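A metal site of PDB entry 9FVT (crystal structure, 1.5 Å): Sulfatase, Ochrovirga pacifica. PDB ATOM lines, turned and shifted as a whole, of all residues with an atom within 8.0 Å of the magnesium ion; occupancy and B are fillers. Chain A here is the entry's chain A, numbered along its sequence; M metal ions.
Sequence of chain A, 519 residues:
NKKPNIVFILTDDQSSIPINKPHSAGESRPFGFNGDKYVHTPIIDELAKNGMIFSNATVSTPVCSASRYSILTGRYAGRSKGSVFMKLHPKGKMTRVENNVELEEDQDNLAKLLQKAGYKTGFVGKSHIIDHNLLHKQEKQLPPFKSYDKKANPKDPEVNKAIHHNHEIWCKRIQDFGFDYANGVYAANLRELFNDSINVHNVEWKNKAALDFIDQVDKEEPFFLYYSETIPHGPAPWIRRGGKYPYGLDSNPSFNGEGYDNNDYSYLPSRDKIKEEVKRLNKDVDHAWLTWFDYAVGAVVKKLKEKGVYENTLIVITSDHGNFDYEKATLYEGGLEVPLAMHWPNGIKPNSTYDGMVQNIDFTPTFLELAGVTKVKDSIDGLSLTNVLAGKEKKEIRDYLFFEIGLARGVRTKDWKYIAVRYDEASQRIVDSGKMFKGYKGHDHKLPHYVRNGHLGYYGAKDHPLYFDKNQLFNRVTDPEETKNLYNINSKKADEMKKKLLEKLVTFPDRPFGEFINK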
ATOM      1  N   LEU A  10     -18.527 -12.939  -3.499  1.00  0.00           N
ATOM      2  CA  LEU A  10     -17.181 -12.880  -2.927  1.00  0.00           C
ATOM      3  C   LEU A  10     -16.988 -14.066  -1.985  1.00  0.00           C
ATOM      4  O   LEU A  10     -17.744 -14.182  -0.993  1.00  0.00           O
ATOM      5  CB  LEU A  10     -17.110 -11.545  -2.157  1.00  0.00           C
ATOM      6  CG  LEU A  10     -15.840 -11.129  -1.456  1.00  0.00           C
ATOM      7  CD1 LEU A  10     -14.767 -10.866  -2.530  1.00  0.00           C
ATOM      8  CD2 LEU A  10     -15.999  -9.947  -0.588  1.00  0.00           C
ATOM      9  N   THR A  11     -15.956 -14.870  -2.209  1.00  0.00           N
ATOM     10  CA  THR A  11     -15.493 -15.840  -1.221  1.00  0.00           C
ATOM     11  C   THR A  11     -14.451 -15.224  -0.276  1.00  0.00           C
ATOM     12  O   THR A  11     -14.090 -14.080  -0.446  1.00  0.00           O
ATOM     13  CB  THR A  11     -14.961 -17.100  -1.906  1.00  0.00           C
ATOM     14  OG1 THR A  11     -13.793 -16.714  -2.625  1.00  0.00           O
ATOM     15  CG2 THR A  11     -15.987 -17.754  -2.820  1.00  0.00           C
ATOM     16  N   ASP A  12     -13.995 -16.001   0.728  1.00  0.00           N
ATOM     17  CA  ASP A  12     -13.238 -15.505   1.875  1.00  0.00           C
ATOM     18  C   ASP A  12     -11.966 -16.340   2.036  1.00  0.00           C
ATOM     19  O   ASP A  12     -12.044 -17.521   2.353  1.00  0.00           O
ATOM     20  CB  ASP A  12     -14.154 -15.591   3.087  1.00  0.00           C
ATOM     21  CG  ASP A  12     -13.679 -14.823   4.292  1.00  0.00           C
ATOM     22  OD1 ASP A  12     -12.686 -14.102   4.165  1.00  0.00           O
ATOM     23  OD2 ASP A  12     -14.309 -14.892   5.365  1.00  0.00           O
ATOM     24  N   ASP A  13     -10.808 -15.742   1.768  1.00  0.00           N
ATOM     25  CA  ASP A  13      -9.511 -16.418   1.958  1.00  0.00           C
ATOM     26  C   ASP A  13      -9.265 -17.501   0.885  1.00  0.00           C
ATOM     27  O   ASP A  13      -8.624 -18.509   1.196  1.00  0.00           O
ATOM     28  CB  ASP A  13      -9.339 -16.996   3.355  1.00  0.00           C
ATOM     29  CG  ASP A  13      -9.164 -16.056   4.528  1.00  0.00           C
ATOM     30  OD1 ASP A  13      -9.565 -14.925   4.448  1.00  0.00           O
ATOM     31  OD2 ASP A  13      -8.632 -16.483   5.563  1.00  0.00           O
ATOM     32  N   GLN A  14      -9.620 -17.217  -0.366  1.00  0.00           N
ATOM     33  CA  GLN A  14      -9.467 -18.151  -1.466  1.00  0.00           C
ATOM     34  C   GLN A  14      -8.506 -17.578  -2.506  1.00  0.00           C
ATOM     35  O   GLN A  14      -8.855 -16.751  -3.342  1.00  0.00           O
ATOM     36  CB  GLN A  14     -10.799 -18.498  -2.096  1.00  0.00           C
ATOM     37  CG  GLN A  14     -10.714 -19.566  -3.156  1.00  0.00           C
ATOM     38  CD  GLN A  14     -12.025 -19.784  -3.847  1.00  0.00           C
ATOM     39  OE1 GLN A  14     -12.894 -18.892  -3.938  1.00  0.00           O
ATOM     40  NE2 GLN A  14     -12.137 -20.941  -4.484  1.00  0.00           N
ATOM     41  N   PRO A  62      -4.128  -7.557   1.732  1.00  0.00           N
ATOM     42  CA  PRO A  62      -4.567  -8.961   1.806  1.00  0.00           C
ATOM     43  C   PRO A  62      -5.029  -9.426   3.167  1.00  0.00           C
ATOM     44  O   PRO A  62      -4.541 -10.411   3.724  1.00  0.00           O
ATOM     45  CB  PRO A  62      -3.347  -9.755   1.306  1.00  0.00           C
ATOM     46  CG  PRO A  62      -2.245  -8.901   1.789  1.00  0.00           C
ATOM     47  CD  PRO A  62      -2.657  -7.448   1.565  1.00  0.00           C
ATOM     48  N   VAL A  63      -6.019  -8.722   3.693  1.00  0.00           N
ATOM     49  CA  VAL A  63      -6.649  -9.167   4.958  1.00  0.00           C
ATOM     50  C   VAL A  63      -8.097  -8.694   4.862  1.00  0.00           C
ATOM     51  O   VAL A  63      -8.337  -7.643   4.376  1.00  0.00           O
ATOM     52  CB  VAL A  63      -5.959  -8.738   6.260  1.00  0.00           C
ATOM     53  CG1 VAL A  63      -6.310  -7.328   6.694  1.00  0.00           C
ATOM     54  CG2 VAL A  63      -6.231  -9.747   7.370  1.00  0.00           C
ATOM     55  N   CYS A  64      -8.988  -9.511   5.368  1.00  0.00           N
ATOM     56  CA  CYS A  64     -10.427  -9.293   5.231  1.00  0.00           C
ATOM     57  C   CYS A  64     -11.015  -7.874   5.341  1.00  0.00           C
ATOM     58  O   CYS A  64     -11.545  -7.444   4.352  1.00  0.00           O
ATOM     59  CB  CYS A  64     -11.017 -10.181   6.285  1.00  0.00           C
ATOM     60  SG  CYS A  64     -12.759 -10.093   6.036  1.00  0.00           S
ATOM     61  N   SER A  65     -10.972  -7.206   6.488  1.00  0.00           N
ATOM     62  CA  SER A  65     -11.674  -5.903   6.617  1.00  0.00           C
ATOM     63  C   SER A  65     -11.130  -4.924   5.569  1.00  0.00           C
ATOM     64  O   SER A  65     -11.887  -4.175   5.051  1.00  0.00           O
ATOM     65  CB  SER A  65     -11.535  -5.301   7.993  1.00  0.00           C
ATOM     66  OG  SER A  65     -12.013  -6.182   8.999  1.00  0.00           O
ATOM     67  N   SER A  67      -9.534  -5.457   2.629  1.00  0.00           N
ATOM     68  CA  SER A  67      -9.916  -5.786   1.264  1.00  0.00           C
ATOM     69  C   SER A  67     -11.372  -5.385   0.985  1.00  0.00           C
ATOM     70  O   SER A  67     -11.664  -4.776  -0.036  1.00  0.00           O
ATOM     71  CB  SER A  67      -9.705  -7.221   0.932  1.00  0.00           C
ATOM     72  OG  SER A  67     -10.126  -7.466  -0.401  1.00  0.00           O
ATOM     73  N   ARG A  68     -12.245  -5.752   1.886  1.00  0.00           N
ATOM     74  CA  ARG A  68     -13.674  -5.460   1.775  1.00  0.00           C
ATOM     75  C   ARG A  68     -13.934  -3.975   1.741  1.00  0.00           C
ATOM     76  O   ARG A  68     -14.772  -3.504   0.956  1.00  0.00           O
ATOM     77  CB  ARG A  68     -14.415  -6.267   2.833  1.00  0.00           C
ATOM     78  CG  ARG A  68     -14.349  -7.767   2.594  1.00  0.00           C
ATOM     79  CD  ARG A  68     -14.519  -8.570   3.862  1.00  0.00           C
ATOM     80  NE  ARG A  68     -14.232  -9.977   3.625  1.00  0.00           N
ATOM     81  CZ  ARG A  68     -15.026 -10.860   3.097  1.00  0.00           C
ATOM     82  NH1 ARG A  68     -16.298 -10.499   2.899  1.00  0.00           N
ATOM     83  NH2 ARG A  68     -14.587 -12.052   2.806  1.00  0.00           N
ATOM     84  N   ASN A  99      -7.397  -5.876  10.294  1.00  0.00           N
ATOM     85  CA  ASN A  99      -8.855  -5.990  10.388  1.00  0.00           C
ATOM     86  C   ASN A  99      -9.394  -4.860  11.273  1.00  0.00           C
ATOM     87  O   ASN A  99     -10.030  -5.130  12.278  1.00  0.00           O
ATOM     88  CB  ASN A  99      -9.306  -7.386  10.820  1.00  0.00           C
ATOM     89  CG  ASN A  99      -9.146  -8.473   9.775  1.00  0.00           C
ATOM     90  OD1 ASN A  99      -9.289  -8.242   8.556  1.00  0.00           O
ATOM     91  ND2 ASN A  99      -8.878  -9.675  10.236  1.00  0.00           N
ATOM     92  N   LYS A 126     -21.076 -12.133   5.090  1.00  0.00           N
ATOM     93  CA  LYS A 126     -20.089 -11.604   5.994  1.00  0.00           C
ATOM     94  C   LYS A 126     -19.823 -10.117   5.752  1.00  0.00           C
ATOM     95  O   LYS A 126     -19.615  -9.665   4.613  1.00  0.00           O
ATOM     96  CB  LYS A 126     -18.782 -12.389   5.754  1.00  0.00           C
ATOM     97  CG  LYS A 126     -17.610 -11.743   6.428  1.00  0.00           C
ATOM     98  CD  LYS A 126     -16.311 -12.584   6.333  1.00  0.00           C
ATOM     99  CE  LYS A 126     -15.114 -11.781   6.712  1.00  0.00           C
ATOM    100  NZ  LYS A 126     -13.880 -12.573   6.713  1.00  0.00           N
ATOM    101  N   HIS A 128     -17.668  -7.585   8.373  1.00  0.00           N
ATOM    102  CA  HIS A 128     -16.326  -7.259   8.845  1.00  0.00           C
ATOM    103  C   HIS A 128     -15.916  -5.804   8.604  1.00  0.00           C
ATOM    104  O   HIS A 128     -14.774  -5.433   8.888  1.00  0.00           O
ATOM    105  CB  HIS A 128     -15.290  -8.224   8.260  1.00  0.00           C
ATOM    106  CG  HIS A 128     -14.250  -8.600   9.255  1.00  0.00           C
ATOM    107  ND1 HIS A 128     -13.242  -9.497   8.914  1.00  0.00           N
ATOM    108  CD2 HIS A 128     -14.055  -8.247  10.573  1.00  0.00           C
ATOM    109  CE1 HIS A 128     -12.468  -9.670  10.004  1.00  0.00           C
ATOM    110  NE2 HIS A 128     -12.950  -8.952  11.027  1.00  0.00           N
ATOM    111  N   ASN A 189     -16.431 -13.024  11.445  1.00  0.00           N
ATOM    112  CA  ASN A 189     -16.232 -14.411  11.099  1.00  0.00           C
ATOM    113  C   ASN A 189     -17.105 -15.313  11.976  1.00  0.00           C
ATOM    114  O   ASN A 189     -17.754 -14.834  12.915  1.00  0.00           O
ATOM    115  CB  ASN A 189     -14.756 -14.802  11.210  1.00  0.00           C
ATOM    116  CG  ASN A 189     -13.866 -13.980  10.293  1.00  0.00           C
ATOM    117  OD1 ASN A 189     -12.880 -13.373  10.730  1.00  0.00           O
ATOM    118  ND2 ASN A 189     -14.213 -13.974   9.040  1.00  0.00           N
ATOM    119  N   GLU A 229     -19.694 -14.591   1.043  1.00  0.00           N
ATOM    120  CA  GLU A 229     -19.579 -15.904   1.699  1.00  0.00           C
ATOM    121  C   GLU A 229     -18.659 -15.861   2.918  1.00  0.00           C
ATOM    122  O   GLU A 229     -17.831 -14.961   3.089  1.00  0.00           O
ATOM    123  CB  GLU A 229     -19.131 -16.957   0.684  1.00  0.00           C
ATOM    124  CG  GLU A 229     -20.240 -17.879   0.184  1.00  0.00           C
ATOM    125  CD  GLU A 229     -20.881 -18.727   1.276  1.00  0.00           C
ATOM    126  OE1 GLU A 229     -20.289 -18.898   2.380  1.00  0.00           O
ATOM    127  OE2 GLU A 229     -21.999 -19.204   1.025  1.00  0.00           O
ATOM    128  N   THR A 230     -18.826 -16.859   3.787  1.00  0.00           N
ATOM    129  CA  THR A 230     -17.829 -17.179   4.807  1.00  0.00           C
ATOM    130  C   THR A 230     -16.825 -18.211   4.273  1.00  0.00           C
ATOM    131  O   THR A 230     -15.707 -18.288   4.787  1.00  0.00           O
ATOM    132  CB  THR A 230     -18.481 -17.660   6.113  1.00  0.00           C
ATOM    133  OG1 THR A 230     -19.324 -18.792   5.845  1.00  0.00           O
ATOM    134  CG2 THR A 230     -19.289 -16.544   6.757  1.00  0.00           C
ATOM    135  N   ILE A 231     -17.212 -19.031   3.303  1.00  0.00           N
ATOM    136  CA  ILE A 231     -16.347 -20.116   2.840  1.00  0.00           C
ATOM    137  C   ILE A 231     -15.213 -19.522   2.028  1.00  0.00           C
ATOM    138  O   ILE A 231     -15.415 -18.539   1.296  1.00  0.00           O
ATOM    139  CB  ILE A 231     -17.111 -21.180   2.016  1.00  0.00           C
ATOM    140  CG1 ILE A 231     -17.826 -20.536   0.828  1.00  0.00           C
ATOM    141  CG2 ILE A 231     -18.029 -21.978   2.939  1.00  0.00           C
ATOM    142  CD1 ILE A 231     -18.514 -21.513  -0.082  1.00  0.00           C
ATOM    143  N   HIS A 233     -13.088 -19.677   4.700  1.00  0.00           N
ATOM    144  CA  HIS A 233     -12.395 -19.160   5.876  1.00  0.00           C
ATOM    145  C   HIS A 233     -12.447 -20.153   7.034  1.00  0.00           C
ATOM    146  O   HIS A 233     -13.397 -20.919   7.177  1.00  0.00           O
ATOM    147  CB  HIS A 233     -13.011 -17.819   6.295  1.00  0.00           C
ATOM    148  CG  HIS A 233     -12.320 -17.024   7.290  1.00  0.00           C
ATOM    149  ND1 HIS A 233     -12.309 -17.304   8.647  1.00  0.00           N
ATOM    150  CD2 HIS A 233     -11.647 -15.879   7.128  1.00  0.00           C
ATOM    151  CE1 HIS A 233     -11.614 -16.357   9.261  1.00  0.00           C
ATOM    152  NE2 HIS A 233     -11.204 -15.451   8.392  1.00  0.00           N
ATOM    153  N   GLY A 234     -11.445 -20.021   7.911  1.00  0.00           N
ATOM    154  CA  GLY A 234     -11.422 -20.832   9.131  1.00  0.00           C
ATOM    155  C   GLY A 234     -12.714 -20.693   9.915  1.00  0.00           C
ATOM    156  O   GLY A 234     -13.237 -19.587  10.053  1.00  0.00           O
ATOM    157  N   SER A 319     -12.616 -13.341  -4.714  1.00  0.00           N
ATOM    158  CA  SER A 319     -12.351 -13.574  -3.299  1.00  0.00           C
ATOM    159  C   SER A 319     -11.758 -12.307  -2.695  1.00  0.00           C
ATOM    160  O   SER A 319     -11.210 -11.466  -3.420  1.00  0.00           O
ATOM    161  CB  SER A 319     -11.416 -14.725  -3.105  1.00  0.00           C
ATOM    162  OG  SER A 319     -11.440 -15.194  -1.767  1.00  0.00           O
ATOM    163  N   ASP A 320     -11.786 -12.167  -1.365  1.00  0.00           N
ATOM    164  CA  ASP A 320     -11.291 -10.962  -0.731  1.00  0.00           C
ATOM    165  C   ASP A 320      -9.760 -10.923  -0.728  1.00  0.00           C
ATOM    166  O   ASP A 320      -9.194  -9.837  -0.813  1.00  0.00           O
ATOM    167  CB  ASP A 320     -11.882 -10.735   0.645  1.00  0.00           C
ATOM    168  CG  ASP A 320     -11.545 -11.742   1.714  1.00  0.00           C
ATOM    169  OD1 ASP A 320     -11.053 -12.841   1.412  1.00  0.00           O
ATOM    170  OD2 ASP A 320     -11.670 -11.336   2.898  1.00  0.00           O
ATOM    171  N   HIS A 321      -9.082 -12.076  -0.653  1.00  0.00           N
ATOM    172  CA  HIS A 321      -7.629 -12.171  -0.727  1.00  0.00           C
ATOM    173  C   HIS A 321      -7.292 -13.649  -0.635  1.00  0.00           C
ATOM    174  O   HIS A 321      -8.122 -14.496  -0.333  1.00  0.00           O
ATOM    175  CB  HIS A 321      -6.910 -11.390   0.377  1.00  0.00           C
ATOM    176  CG  HIS A 321      -7.303 -11.823   1.761  1.00  0.00           C
ATOM    177  ND1 HIS A 321      -6.802 -12.959   2.357  1.00  0.00           N
ATOM    178  CD2 HIS A 321      -8.235 -11.328   2.637  1.00  0.00           C
ATOM    179  CE1 HIS A 321      -7.446 -13.151   3.521  1.00  0.00           C
ATOM    180  NE2 HIS A 321      -8.266 -12.139   3.727  1.00  0.00           N
ATOM    181  N   GLY A 322      -6.033 -13.969  -0.904  1.00  0.00           N
ATOM    182  CA  GLY A 322      -5.555 -15.326  -0.768  1.00  0.00           C
ATOM    183  C   GLY A 322      -5.103 -15.687   0.635  1.00  0.00           C
ATOM    184  O   GLY A 322      -4.853 -14.875   1.516  1.00  0.00           O
ATOM    185  N   ASN A 323      -4.985 -17.009   0.815  1.00  0.00           N
ATOM    186  CA  ASN A 323      -4.324 -17.569   1.979  1.00  0.00           C
ATOM    187  C   ASN A 323      -3.591 -18.841   1.558  1.00  0.00           C
ATOM    188  O   ASN A 323      -3.694 -19.871   2.199  1.00  0.00           O
ATOM    189  CB  ASN A 323      -5.249 -17.864   3.152  1.00  0.00           C
ATOM    190  CG  ASN A 323      -4.517 -18.219   4.436  1.00  0.00           C
ATOM    191  OD1 ASN A 323      -3.367 -17.821   4.665  1.00  0.00           O
ATOM    192  ND2 ASN A 323      -5.222 -18.964   5.255  1.00  0.00           N
ATOM    193  N   LYS A 328      -1.741 -15.038   3.722  1.00  0.00           N
ATOM    194  CA  LYS A 328      -2.640 -14.014   4.184  1.00  0.00           C
ATOM    195  C   LYS A 328      -1.905 -12.990   5.065  1.00  0.00           C
ATOM    196  O   LYS A 328      -1.039 -13.358   5.862  1.00  0.00           O
ATOM    197  CB  LYS A 328      -3.719 -14.702   5.026  1.00  0.00           C
ATOM    198  CG  LYS A 328      -4.729 -13.797   5.723  1.00  0.00           C
ATOM    199  CD  LYS A 328      -5.800 -14.605   6.454  1.00  0.00           C
ATOM    200  CE  LYS A 328      -6.926 -13.840   7.089  1.00  0.00           C
ATOM    201  NZ  LYS A 328      -7.939 -14.760   7.619  1.00  0.00           N
HETATM  202 MG    MG M   1     -10.734 -13.041   4.259  1.00  0.00          MG
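The side-chain carboxylate (OD1) of Asp 12 is bound to the magnesium ion (2.2 Å).
The side-chain carboxylate (OD1) of Asp 13 is bound to the magnesium ion (2.2 Å).
OD2 of Asp 320 is bound to the magnesium ion (2.4 Å).
The magnesium ion has three donor atoms within binding distance.
Slightly farther from the magnesium ion lies NE2 of His 321 (2.7 Å).
The backbone carbonyl oxygen (O) of Asp 12 is in hydrogen-bond range of the backbone NH (N) of His 233 (3.4 Å).
A ring nitrogen (NE2) of His 321 sits close to the side-chain carboxylate of Asp 13 (3.2 Å).
The side-chain sulfur (SG) of Cys 64 lies close to the side-chain carboxylate (OD2) of Asp 320.
OD1 of Asp 320 is in salt-bridge range of NH2 of Arg 68.
The backbone NH (N) of Asp 320 sits at hydrogen-bond distance from the backbone carbonyl oxygen (O) of Thr 11 (3.1 Å).
A ring nitrogen (NE2) of His 321 is in hydrogen-bond range of the backbone NH (N) of Cys 64 (3.2 Å).
The side-chain sulfur (SG) of Cys 64 is in hydrogen-bond range of the side-chain amino group (NZ) of Lys 126, 2.8 Å away.
OD1 of Asn 99 sits at hydrogen-bond distance from N of Cys 64.
Cys 64 touches the magnesium ion.
Of the 26 residues printed, 5 come within 4 Å of the magnesium ion.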
